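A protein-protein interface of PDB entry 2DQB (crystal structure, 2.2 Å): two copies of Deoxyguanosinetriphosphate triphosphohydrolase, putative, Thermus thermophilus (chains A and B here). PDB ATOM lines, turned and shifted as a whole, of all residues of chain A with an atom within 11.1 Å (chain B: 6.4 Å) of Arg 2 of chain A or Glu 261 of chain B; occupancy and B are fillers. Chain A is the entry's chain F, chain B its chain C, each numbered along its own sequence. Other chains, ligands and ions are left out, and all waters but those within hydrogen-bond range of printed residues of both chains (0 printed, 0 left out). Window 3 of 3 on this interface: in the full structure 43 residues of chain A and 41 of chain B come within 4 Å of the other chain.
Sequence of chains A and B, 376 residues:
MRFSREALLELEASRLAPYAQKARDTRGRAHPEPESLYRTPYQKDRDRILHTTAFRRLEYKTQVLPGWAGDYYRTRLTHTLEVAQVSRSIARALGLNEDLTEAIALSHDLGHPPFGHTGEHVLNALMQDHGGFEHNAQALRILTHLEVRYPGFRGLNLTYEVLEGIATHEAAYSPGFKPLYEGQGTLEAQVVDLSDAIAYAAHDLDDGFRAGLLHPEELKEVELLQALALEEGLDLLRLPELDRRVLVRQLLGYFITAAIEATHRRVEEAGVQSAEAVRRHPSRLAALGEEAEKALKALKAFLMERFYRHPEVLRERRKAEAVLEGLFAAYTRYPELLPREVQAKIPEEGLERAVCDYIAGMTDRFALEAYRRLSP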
ATOM      1  N   MET A   1     -22.392   5.351 -26.667  1.00  0.00           N
ATOM      2  CA  MET A   1     -22.911   6.165 -25.529  1.00  0.00           C
ATOM      3  C   MET A   1     -23.652   7.371 -26.110  1.00  0.00           C
ATOM      4  O   MET A   1     -23.111   8.121 -26.922  1.00  0.00           O
ATOM      5  CB  MET A   1     -21.734   6.604 -24.641  1.00  0.00           C
ATOM      6  CG  MET A   1     -22.100   7.144 -23.267  1.00  0.00           C
ATOM      7  SD  MET A   1     -20.719   6.727 -21.946  1.00  0.00           S
ATOM      8  CE  MET A   1     -19.908   8.429 -21.657  1.00  0.00           C
ATOM      9  N   ARG A   2     -24.904   7.544 -25.715  1.00  0.00           N
ATOM     10  CA  ARG A   2     -25.686   8.653 -26.232  1.00  0.00           C
ATOM     11  C   ARG A   2     -26.200   9.552 -25.130  1.00  0.00           C
ATOM     12  O   ARG A   2     -27.122   9.185 -24.401  1.00  0.00           O
ATOM     13  CB  ARG A   2     -26.868   8.133 -27.033  1.00  0.00           C
ATOM     14  CG  ARG A   2     -26.486   7.314 -28.257  1.00  0.00           C
ATOM     15  CD  ARG A   2     -27.668   6.476 -28.707  1.00  0.00           C
ATOM     16  NE  ARG A   2     -28.045   5.500 -27.686  1.00  0.00           N
ATOM     17  CZ  ARG A   2     -29.034   4.615 -27.815  1.00  0.00           C
ATOM     18  NH1 ARG A   2     -29.761   4.577 -28.933  1.00  0.00           N
ATOM     19  NH2 ARG A   2     -29.299   3.765 -26.822  1.00  0.00           N
ATOM     20  N   PHE A   3     -25.607  10.732 -25.018  1.00  0.00           N
ATOM     21  CA  PHE A   3     -26.022  11.698 -24.012  1.00  0.00           C
ATOM     22  C   PHE A   3     -27.285  12.454 -24.389  1.00  0.00           C
ATOM     23  O   PHE A   3     -27.265  13.342 -25.242  1.00  0.00           O
ATOM     24  CB  PHE A   3     -24.902  12.691 -23.753  1.00  0.00           C
ATOM     25  CG  PHE A   3     -23.672  12.062 -23.202  1.00  0.00           C
ATOM     26  CD1 PHE A   3     -22.904  11.215 -23.985  1.00  0.00           C
ATOM     27  CD2 PHE A   3     -23.299  12.288 -21.882  1.00  0.00           C
ATOM     28  CE1 PHE A   3     -21.784  10.606 -23.467  1.00  0.00           C
ATOM     29  CE2 PHE A   3     -22.181  11.688 -21.345  1.00  0.00           C
ATOM     30  CZ  PHE A   3     -21.419  10.846 -22.138  1.00  0.00           C
ATOM     31  N   SER A   4     -28.388  12.100 -23.749  1.00  0.00           N
ATOM     32  CA  SER A   4     -29.665  12.761 -23.996  1.00  0.00           C
ATOM     33  C   SER A   4     -29.630  14.182 -23.433  1.00  0.00           C
ATOM     34  O   SER A   4     -28.715  14.547 -22.700  1.00  0.00           O
ATOM     35  CB  SER A   4     -30.780  12.020 -23.273  1.00  0.00           C
ATOM     36  OG  SER A   4     -30.675  12.295 -21.880  1.00  0.00           O
ATOM     37  N   ARG A   5     -30.640  14.979 -23.773  1.00  0.00           N
ATOM     38  CA  ARG A   5     -30.745  16.332 -23.237  1.00  0.00           C
ATOM     39  C   ARG A   5     -30.802  16.188 -21.713  1.00  0.00           C
ATOM     40  O   ARG A   5     -29.968  16.752 -20.991  1.00  0.00           O
ATOM     41  CB  ARG A   5     -32.022  17.013 -23.746  1.00  0.00           C
ATOM     42  CG  ARG A   5     -32.394  18.304 -23.006  1.00  0.00           C
ATOM     43  CD  ARG A   5     -33.624  18.961 -23.633  1.00  0.00           C
ATOM     44  NE  ARG A   5     -34.783  18.069 -23.682  1.00  0.00           N
ATOM     45  CZ  ARG A   5     -35.598  17.831 -22.654  1.00  0.00           C
ATOM     46  NH1 ARG A   5     -35.388  18.421 -21.482  1.00  0.00           N
ATOM     47  NH2 ARG A   5     -36.628  17.003 -22.799  1.00  0.00           N
ATOM     48  N   GLU A   6     -31.777  15.414 -21.229  1.00  0.00           N
ATOM     49  CA  GLU A   6     -31.925  15.186 -19.789  1.00  0.00           C
ATOM     50  C   GLU A   6     -30.555  14.937 -19.204  1.00  0.00           C
ATOM     51  O   GLU A   6     -30.169  15.529 -18.193  1.00  0.00           O
ATOM     52  CB  GLU A   6     -32.791  13.959 -19.509  1.00  0.00           C
ATOM     53  CG  GLU A   6     -34.230  14.070 -19.969  1.00  0.00           C
ATOM     54  CD  GLU A   6     -34.861  15.387 -19.573  1.00  0.00           C
ATOM     55  OE1 GLU A   6     -34.527  15.917 -18.480  1.00  0.00           O
ATOM     56  OE2 GLU A   6     -35.700  15.884 -20.357  1.00  0.00           O
ATOM     57  N   ALA A   7     -29.816  14.056 -19.866  1.00  0.00           N
ATOM     58  CA  ALA A   7     -28.475  13.709 -19.438  1.00  0.00           C
ATOM     59  C   ALA A   7     -27.571  14.945 -19.370  1.00  0.00           C
ATOM     60  O   ALA A   7     -26.915  15.193 -18.361  1.00  0.00           O
ATOM     61  CB  ALA A   7     -27.897  12.657 -20.393  1.00  0.00           C
ATOM     62  N   LEU A   8     -27.538  15.738 -20.438  1.00  0.00           N
ATOM     63  CA  LEU A   8     -26.685  16.934 -20.453  1.00  0.00           C
ATOM     64  C   LEU A   8     -27.109  17.908 -19.353  1.00  0.00           C
ATOM     65  O   LEU A   8     -26.267  18.477 -18.651  1.00  0.00           O
ATOM     66  CB  LEU A   8     -26.756  17.625 -21.825  1.00  0.00           C
ATOM     67  CG  LEU A   8     -26.436  16.770 -23.063  1.00  0.00           C
ATOM     68  CD1 LEU A   8     -26.751  17.578 -24.319  1.00  0.00           C
ATOM     69  CD2 LEU A   8     -24.973  16.317 -23.059  1.00  0.00           C
ATOM     70  N   LEU A   9     -28.420  18.095 -19.202  1.00  0.00           N
ATOM     71  CA  LEU A   9     -28.947  18.994 -18.168  1.00  0.00           C
ATOM     72  C   LEU A   9     -28.441  18.587 -16.779  1.00  0.00           C
ATOM     73  O   LEU A   9     -28.015  19.426 -15.977  1.00  0.00           O
ATOM     74  CB  LEU A   9     -30.477  18.971 -18.185  1.00  0.00           C
ATOM     75  CG  LEU A   9     -31.160  19.676 -19.359  1.00  0.00           C
ATOM     76  CD1 LEU A   9     -32.669  19.495 -19.270  1.00  0.00           C
ATOM     77  CD2 LEU A   9     -30.792  21.148 -19.350  1.00  0.00           C
ATOM     78  N   LEU A  11     -25.761  16.759 -16.104  1.00  0.00           N
ATOM     79  CA  LEU A  11     -24.323  16.992 -16.019  1.00  0.00           C
ATOM     80  C   LEU A  11     -24.003  18.444 -15.712  1.00  0.00           C
ATOM     81  O   LEU A  11     -23.227  18.757 -14.810  1.00  0.00           O
ATOM     82  CB  LEU A  11     -23.640  16.609 -17.328  1.00  0.00           C
ATOM     83  CG  LEU A  11     -23.502  15.118 -17.607  1.00  0.00           C
ATOM     84  CD1 LEU A  11     -22.791  14.931 -18.937  1.00  0.00           C
ATOM     85  CD2 LEU A  11     -22.716  14.461 -16.486  1.00  0.00           C
ATOM     86  N   SER A  36     -34.348  19.069 -28.546  1.00  0.00           N
ATOM     87  CA  SER A  36     -35.258  18.500 -27.554  1.00  0.00           C
ATOM     88  C   SER A  36     -34.795  17.115 -27.096  1.00  0.00           C
ATOM     89  O   SER A  36     -34.797  16.812 -25.901  1.00  0.00           O
ATOM     90  CB  SER A  36     -36.679  18.403 -28.124  1.00  0.00           C
ATOM     91  OG  SER A  36     -37.598  17.984 -27.127  1.00  0.00           O
ATOM     92  N   LEU A  37     -34.393  16.276 -28.047  1.00  0.00           N
ATOM     93  CA  LEU A  37     -33.926  14.933 -27.720  1.00  0.00           C
ATOM     94  C   LEU A  37     -32.464  14.941 -27.240  1.00  0.00           C
ATOM     95  O   LEU A  37     -32.160  14.457 -26.143  1.00  0.00           O
ATOM     96  CB  LEU A  37     -34.066  14.018 -28.941  1.00  0.00           C
ATOM     97  CG  LEU A  37     -35.422  13.884 -29.662  1.00  0.00           C
ATOM     98  CD1 LEU A  37     -36.461  13.260 -28.732  1.00  0.00           C
ATOM     99  CD2 LEU A  37     -35.886  15.256 -30.165  1.00  0.00           C
ATOM    100  N   TYR A  38     -31.567  15.506 -28.051  1.00  0.00           N
ATOM    101  CA  TYR A  38     -30.137  15.563 -27.718  1.00  0.00           C
ATOM    102  C   TYR A  38     -29.577  16.908 -27.278  1.00  0.00           C
ATOM    103  O   TYR A  38     -28.614  16.958 -26.515  1.00  0.00           O
ATOM    104  CB  TYR A  38     -29.305  15.069 -28.906  1.00  0.00           C
ATOM    105  CG  TYR A  38     -29.440  13.588 -29.148  1.00  0.00           C
ATOM    106  CD1 TYR A  38     -28.959  12.668 -28.211  1.00  0.00           C
ATOM    107  CD2 TYR A  38     -30.100  13.100 -30.271  1.00  0.00           C
ATOM    108  CE1 TYR A  38     -29.140  11.307 -28.381  1.00  0.00           C
ATOM    109  CE2 TYR A  38     -30.288  11.734 -30.450  1.00  0.00           C
ATOM    110  CZ  TYR A  38     -29.809  10.840 -29.493  1.00  0.00           C
ATOM    111  OH  TYR A  38     -30.041   9.485 -29.616  1.00  0.00           O
ATOM    112  N   ARG A  39     -30.176  17.996 -27.743  1.00  0.00           N
ATOM    113  CA  ARG A  39     -29.681  19.341 -27.429  1.00  0.00           C
ATOM    114  C   ARG A  39     -30.222  19.995 -26.154  1.00  0.00           C
ATOM    115  O   ARG A  39     -31.355  19.761 -25.742  1.00  0.00           O
ATOM    116  CB  ARG A  39     -29.958  20.273 -28.629  1.00  0.00           C
ATOM    117  CG  ARG A  39     -29.396  19.752 -29.959  1.00  0.00           C
ATOM    118  CD  ARG A  39     -29.666  20.689 -31.138  1.00  0.00           C
ATOM    119  NE  ARG A  39     -31.095  20.901 -31.357  1.00  0.00           N
ATOM    120  CZ  ARG A  39     -31.602  21.777 -32.226  1.00  0.00           C
ATOM    121  NH1 ARG A  39     -32.916  21.903 -32.351  1.00  0.00           N
ATOM    122  NH2 ARG A  39     -30.801  22.526 -32.970  1.00  0.00           N
ATOM    123  N   GLN A  43     -28.101  25.177 -26.501  1.00  0.00           N
ATOM    124  CA  GLN A  43     -27.437  24.570 -27.643  1.00  0.00           C
ATOM    125  C   GLN A  43     -28.328  24.899 -28.845  1.00  0.00           C
ATOM    126  O   GLN A  43     -27.870  25.421 -29.879  1.00  0.00           O
ATOM    127  CB  GLN A  43     -27.397  23.066 -27.464  1.00  0.00           C
ATOM    128  CG  GLN A  43     -26.176  22.397 -27.966  1.00  0.00           C
ATOM    129  CD  GLN A  43     -26.253  20.913 -27.746  1.00  0.00           C
ATOM    130  OE1 GLN A  43     -26.731  20.459 -26.703  1.00  0.00           O
ATOM    131  NE2 GLN A  43     -25.783  20.141 -28.720  1.00  0.00           N
ATOM    132  N   TYR B  19     -14.187   6.177 -24.549  1.00  0.00           N
ATOM    133  CA  TYR B  19     -13.509   6.137 -25.838  1.00  0.00           C
ATOM    134  C   TYR B  19     -13.107   7.527 -26.362  1.00  0.00           C
ATOM    135  O   TYR B  19     -12.452   7.623 -27.401  1.00  0.00           O
ATOM    136  CB  TYR B  19     -14.394   5.409 -26.867  1.00  0.00           C
ATOM    137  CG  TYR B  19     -15.832   5.884 -26.893  1.00  0.00           C
ATOM    138  CD1 TYR B  19     -16.158   7.159 -27.362  1.00  0.00           C
ATOM    139  CD2 TYR B  19     -16.862   5.068 -26.433  1.00  0.00           C
ATOM    140  CE1 TYR B  19     -17.451   7.613 -27.368  1.00  0.00           C
ATOM    141  CE2 TYR B  19     -18.173   5.503 -26.438  1.00  0.00           C
ATOM    142  CZ  TYR B  19     -18.464   6.792 -26.904  1.00  0.00           C
ATOM    143  OH  TYR B  19     -19.755   7.278 -26.851  1.00  0.00           O
ATOM    144  N   ARG B  92     -20.834  16.130 -28.702  1.00  0.00           N
ATOM    145  CA  ARG B  92     -21.482  16.216 -27.403  1.00  0.00           C
ATOM    146  C   ARG B  92     -22.410  15.035 -27.186  1.00  0.00           C
ATOM    147  O   ARG B  92     -22.389  14.419 -26.122  1.00  0.00           O
ATOM    148  CB  ARG B  92     -22.274  17.520 -27.259  1.00  0.00           C
ATOM    149  CG  ARG B  92     -22.856  17.715 -25.855  1.00  0.00           C
ATOM    150  CD  ARG B  92     -23.435  19.119 -25.633  1.00  0.00           C
ATOM    151  NE  ARG B  92     -22.425  20.176 -25.716  1.00  0.00           N
ATOM    152  CZ  ARG B  92     -22.664  21.463 -25.471  1.00  0.00           C
ATOM    153  NH1 ARG B  92     -23.883  21.853 -25.117  1.00  0.00           N
ATOM    154  NH2 ARG B  92     -21.695  22.362 -25.602  1.00  0.00           N
ATOM    155  N   ALA B  93     -23.211  14.698 -28.193  1.00  0.00           N
ATOM    156  CA  ALA B  93     -24.136  13.578 -28.045  1.00  0.00           C
ATOM    157  C   ALA B  93     -23.426  12.249 -27.776  1.00  0.00           C
ATOM    158  O   ALA B  93     -24.015  11.346 -27.182  1.00  0.00           O
ATOM    159  CB  ALA B  93     -25.027  13.453 -29.287  1.00  0.00           C
ATOM    160  N   LEU B  94     -22.169  12.128 -28.199  1.00  0.00           N
ATOM    161  CA  LEU B  94     -21.433  10.882 -27.994  1.00  0.00           C
ATOM    162  C   LEU B  94     -20.433  10.941 -26.843  1.00  0.00           C
ATOM    163  O   LEU B  94     -19.674  10.002 -26.630  1.00  0.00           O
ATOM    164  CB  LEU B  94     -20.706  10.477 -29.287  1.00  0.00           C
ATOM    165  CG  LEU B  94     -21.570  10.208 -30.523  1.00  0.00           C
ATOM    166  CD1 LEU B  94     -20.678  10.011 -31.735  1.00  0.00           C
ATOM    167  CD2 LEU B  94     -22.455   8.999 -30.312  1.00  0.00           C
ATOM    168  N   GLY B  95     -20.415  12.052 -26.122  1.00  0.00           N
ATOM    169  CA  GLY B  95     -19.492  12.192 -25.011  1.00  0.00           C
ATOM    170  C   GLY B  95     -18.064  12.358 -25.430  1.00  0.00           C
ATOM    171  O   GLY B  95     -17.130  12.117 -24.646  1.00  0.00           O
ATOM    172  N   ILE B 256     -27.715  14.319 -38.858  1.00  0.00           N
ATOM    173  CA  ILE B 256     -27.059  14.440 -37.554  1.00  0.00           C
ATOM    174  C   ILE B 256     -27.531  13.327 -36.614  1.00  0.00           C
ATOM    175  O   ILE B 256     -26.745  12.765 -35.859  1.00  0.00           O
ATOM    176  CB  ILE B 256     -27.326  15.821 -36.930  1.00  0.00           C
ATOM    177  CG1 ILE B 256     -26.502  16.874 -37.669  1.00  0.00           C
ATOM    178  CG2 ILE B 256     -27.020  15.795 -35.426  1.00  0.00           C
ATOM    179  CD1 ILE B 256     -26.582  18.281 -37.068  1.00  0.00           C
ATOM    180  N   THR B 257     -28.819  13.010 -36.690  1.00  0.00           N
ATOM    181  CA  THR B 257     -29.419  11.957 -35.884  1.00  0.00           C
ATOM    182  C   THR B 257     -28.900  10.575 -36.296  1.00  0.00           C
ATOM    183  O   THR B 257     -28.512   9.773 -35.439  1.00  0.00           O
ATOM    184  CB  THR B 257     -30.932  12.010 -36.007  1.00  0.00           C
ATOM    185  OG1 THR B 257     -31.392  13.180 -35.328  1.00  0.00           O
ATOM    186  CG2 THR B 257     -31.588  10.775 -35.410  1.00  0.00           C
ATOM    187  N   ALA B 258     -28.908  10.302 -37.597  1.00  0.00           N
ATOM    188  CA  ALA B 258     -28.394   9.037 -38.123  1.00  0.00           C
ATOM    189  C   ALA B 258     -26.952   8.884 -37.664  1.00  0.00           C
ATOM    190  O   ALA B 258     -26.534   7.806 -37.232  1.00  0.00           O
ATOM    191  CB  ALA B 258     -28.450   9.031 -39.632  1.00  0.00           C
ATOM    192  N   ALA B 259     -26.202   9.981 -37.733  1.00  0.00           N
ATOM    193  CA  ALA B 259     -24.810   9.984 -37.315  1.00  0.00           C
ATOM    194  C   ALA B 259     -24.597   9.594 -35.831  1.00  0.00           C
ATOM    195  O   ALA B 259     -23.681   8.837 -35.514  1.00  0.00           O
ATOM    196  CB  ALA B 259     -24.196  11.347 -37.577  1.00  0.00           C
ATOM    197  N   ILE B 260     -25.409  10.134 -34.930  1.00  0.00           N
ATOM    198  CA  ILE B 260     -25.261   9.826 -33.510  1.00  0.00           C
ATOM    199  C   ILE B 260     -25.647   8.366 -33.216  1.00  0.00           C
ATOM    200  O   ILE B 260     -24.904   7.636 -32.557  1.00  0.00           O
ATOM    201  CB  ILE B 260     -26.108  10.799 -32.666  1.00  0.00           C
ATOM    202  CG1 ILE B 260     -25.486  12.199 -32.747  1.00  0.00           C
ATOM    203  CG2 ILE B 260     -26.196  10.330 -31.229  1.00  0.00           C
ATOM    204  CD1 ILE B 260     -26.457  13.320 -32.432  1.00  0.00           C
ATOM    205  N   GLU B 261     -26.792   7.942 -33.733  1.00  0.00           N
ATOM    206  CA  GLU B 261     -27.253   6.577 -33.533  1.00  0.00           C
ATOM    207  C   GLU B 261     -26.327   5.509 -34.147  1.00  0.00           C
ATOM    208  O   GLU B 261     -25.916   4.562 -33.462  1.00  0.00           O
ATOM    209  CB  GLU B 261     -28.670   6.416 -34.098  1.00  0.00           C
ATOM    210  CG  GLU B 261     -29.761   7.160 -33.299  1.00  0.00           C
ATOM    211  CD  GLU B 261     -29.838   6.692 -31.833  1.00  0.00           C
ATOM    212  OE1 GLU B 261     -29.719   5.472 -31.591  1.00  0.00           O
ATOM    213  OE2 GLU B 261     -30.026   7.540 -30.934  1.00  0.00           O
ATOM    214  N   ALA B 262     -25.981   5.674 -35.421  1.00  0.00           N
ATOM    215  CA  ALA B 262     -25.144   4.701 -36.106  1.00  0.00           C
ATOM    216  C   ALA B 262     -23.725   4.635 -35.562  1.00  0.00           C
ATOM    217  O   ALA B 262     -23.141   3.552 -35.458  1.00  0.00           O
ATOM    218  CB  ALA B 262     -25.136   4.977 -37.635  1.00  0.00           C
ATOM    219  N   THR B 263     -23.165   5.784 -35.206  1.00  0.00           N
ATOM    220  CA  THR B 263     -21.813   5.798 -34.662  1.00  0.00           C
ATOM    221  C   THR B 263     -21.844   5.184 -33.268  1.00  0.00           C
ATOM    222  O   THR B 263     -20.898   4.515 -32.840  1.00  0.00           O
ATOM    223  CB  THR B 263     -21.262   7.215 -34.575  1.00  0.00           C
ATOM    224  OG1 THR B 263     -21.177   7.770 -35.904  1.00  0.00           O
ATOM    225  CG2 THR B 263     -19.876   7.208 -33.927  1.00  0.00           C
ATOM    226  N   HIS B 264     -22.931   5.440 -32.557  1.00  0.00           N
ATOM    227  CA  HIS B 264     -23.096   4.880 -31.224  1.00  0.00           C
ATOM    228  C   HIS B 264     -23.129   3.364 -31.354  1.00  0.00           C
ATOM    229  O   HIS B 264     -22.481   2.663 -30.582  1.00  0.00           O
ATOM    230  CB  HIS B 264     -24.401   5.350 -30.587  1.00  0.00           C
ATOM    231  CG  HIS B 264     -24.827   4.517 -29.421  1.00  0.00           C
ATOM    232  ND1 HIS B 264     -24.109   4.460 -28.243  1.00  0.00           N
ATOM    233  CD2 HIS B 264     -25.882   3.683 -29.262  1.00  0.00           C
ATOM    234  CE1 HIS B 264     -24.706   3.626 -27.410  1.00  0.00           C
ATOM    235  NE2 HIS B 264     -25.783   3.142 -28.005  1.00  0.00           N
ATOM    236  N   ARG B 265     -23.884   2.869 -32.336  1.00  0.00           N
ATOM    237  CA  ARG B 265     -23.984   1.431 -32.550  1.00  0.00           C
ATOM    238  C   ARG B 265     -22.647   0.794 -32.900  1.00  0.00           C
ATOM    239  O   ARG B 265     -22.335  -0.279 -32.394  1.00  0.00           O
ATOM    240  CB  ARG B 265     -25.014   1.090 -33.630  1.00  0.00           C
ATOM    241  CG  ARG B 265     -26.459   1.207 -33.159  1.00  0.00           C
ATOM    242  CD  ARG B 265     -27.475   0.675 -34.174  1.00  0.00           C
ATOM    243  NE  ARG B 265     -27.471   1.396 -35.451  1.00  0.00           N
ATOM    244  CZ  ARG B 265     -26.734   1.057 -36.508  1.00  0.00           C
ATOM    245  NH1 ARG B 265     -25.931   0.001 -36.449  1.00  0.00           N
ATOM    246  NH2 ARG B 265     -26.809   1.763 -37.630  1.00  0.00           N
ATOM    247  N   ARG B 266     -21.838   1.439 -33.737  1.00  0.00           N
ATOM    248  CA  ARG B 266     -20.554   0.845 -34.082  1.00  0.00           C
ATOM    249  C   ARG B 266     -19.480   0.992 -33.002  1.00  0.00           C
ATOM    250  O   ARG B 266     -18.519   0.217 -32.962  1.00  0.00           O
ATOM    251  CB  ARG B 266     -20.054   1.367 -35.444  1.00  0.00           C
ATOM    252  CG  ARG B 266     -20.627   0.539 -36.600  1.00  0.00           C
ATOM    253  CD  ARG B 266     -20.011   0.819 -37.981  1.00  0.00           C
ATOM    254  NE  ARG B 266     -18.548   0.713 -38.041  1.00  0.00           N
ATOM    255  CZ  ARG B 266     -17.820  -0.286 -37.541  1.00  0.00           C
ATOM    256  NH1 ARG B 266     -16.499  -0.261 -37.669  1.00  0.00           N
ATOM    257  NH2 ARG B 266     -18.397  -1.297 -36.898  1.00  0.00           N
ATOM    258  N   ALA B 287     -20.194   7.061 -38.330  1.00  0.00           N
ATOM    259  CA  ALA B 287     -21.000   6.593 -39.451  1.00  0.00           C
ATOM    260  C   ALA B 287     -22.410   7.121 -39.463  1.00  0.00           C
ATOM    261  O   ALA B 287     -22.882   7.706 -38.481  1.00  0.00           O
ATOM    262  CB  ALA B 287     -21.045   5.061 -39.466  1.00  0.00           C
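Met 1 of chain A touches Leu 94 of chain B (O to CA, 3.4 Å).
Arg 2 of chain A touches Ala 93 of chain B.
CB of Phe 3 of chain A touches O of Arg 92 of chain B, at 3.9 Å.
Phe 3 of chain A touches Leu 94 of chain B (CE1 to C, 3.7 Å).
Gly 95 of chain B touches Phe 3 of chain A (CA to CE1, 3.2 Å).
Leu 8 of chain A touches Arg 92 of chain B.
NH1 of Arg 92 of chain B touches OE1 of Gln 43 of chain A, 3.5 Å away.
Of chain B, only Ala 93, Glu 261 and His 264 come within 4 Å of Arg 2 of chain A.
Of the printed residues of chain A, Glu 261 of chain B touches Arg 2 (2.8 Å) and Tyr 38 (2.3 Å).
Ala 93 of chain B touches just these residues of chain A: Met 1 (3.4 Å), Arg 2 (3.3 Å) and Phe 3 (2.8 Å).
No residue of chain A comes within 4 Å of Ala 258 of chain B.
No residue of chain A comes within 4 Å of Ala 259 of chain B.
No residue of chain A comes within 4 Å of Ala 262 of chain B.
No residue of chain A comes within 4 Å of Thr 263 of chain B.
Of chain A, only Met 1 and Arg 2 come within 4 Å of His 264 of chain B.
No residue of chain A comes within 4 Å of Arg 265 of chain B.
Of the printed residues of chain B, Tyr 38 of chain A touches Glu 261 (2.3 Å).
Of the printed residues of chain B, Phe 3 of chain A touches Arg 92, Ala 93, Leu 94 and Gly 95.
Of the printed residues of chain B, Gln 43 of chain A touches Arg 92.
Ala 287 of chain B touches none of the printed residues of chain A.
Leu 11 of chain A touches none of the printed residues of chain B.
Of the 15 printed residues of chain A, 6 touch a printed residue of chain B.
Printed residues of chain A that touch a printed residue of chain B: Met 1, Arg 2, Phe 3, Leu 8, Tyr 38 and Gln 43.
Hydrophobic or aromatic side chains of chain A that line the printed part of chain B: Met 1, Phe 3, Leu 8 and Tyr 38.
Printed residues of chain B that touch a printed residue of chain A: Tyr 19, Arg 92, Ala 93, Leu 94, Gly 95, Glu 261 and His 264.
Among the printed residues, 14 pairs touch across the chains.
No position is printed for both chains.
Of the 14 pairs that touch across the chains among the printed residues, none has its exchanged pair printed and touching as well.
OH of Tyr 19 of chain B lies within hydrogen-bond range of O of Leu 94 of chain B, at 2.7 Å.
The backbone NH (N) of Phe 3 of chain A is in hydrogen-bond range of the backbone carbonyl oxygen (O) of Ala 93 of chain B, 2.8 Å away.
A ring nitrogen (ND1) of His 264 of chain B lies within hydrogen-bond range of the backbone NH of Met 1 of chain A, 2.5 Å away.
O of Met 1 of chain A sits close to O of Ala 93 of chain B (3.4 Å).
OH of Tyr 38 of chain A lies close to OE2 of Glu 261 of chain B, 2.3 Å away.
The guanidinium group of Arg 2 of chain A lies within salt-bridge range of the side-chain carboxylate of Glu 261 of chain B (2.8 Å).
NE of Arg 2 of chain A lies close to NE2 of His 264 of chain B, at 3.3 Å.
OH of Tyr 19 of chain B sits close to N of Met 1 of chain A (3.3 Å).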
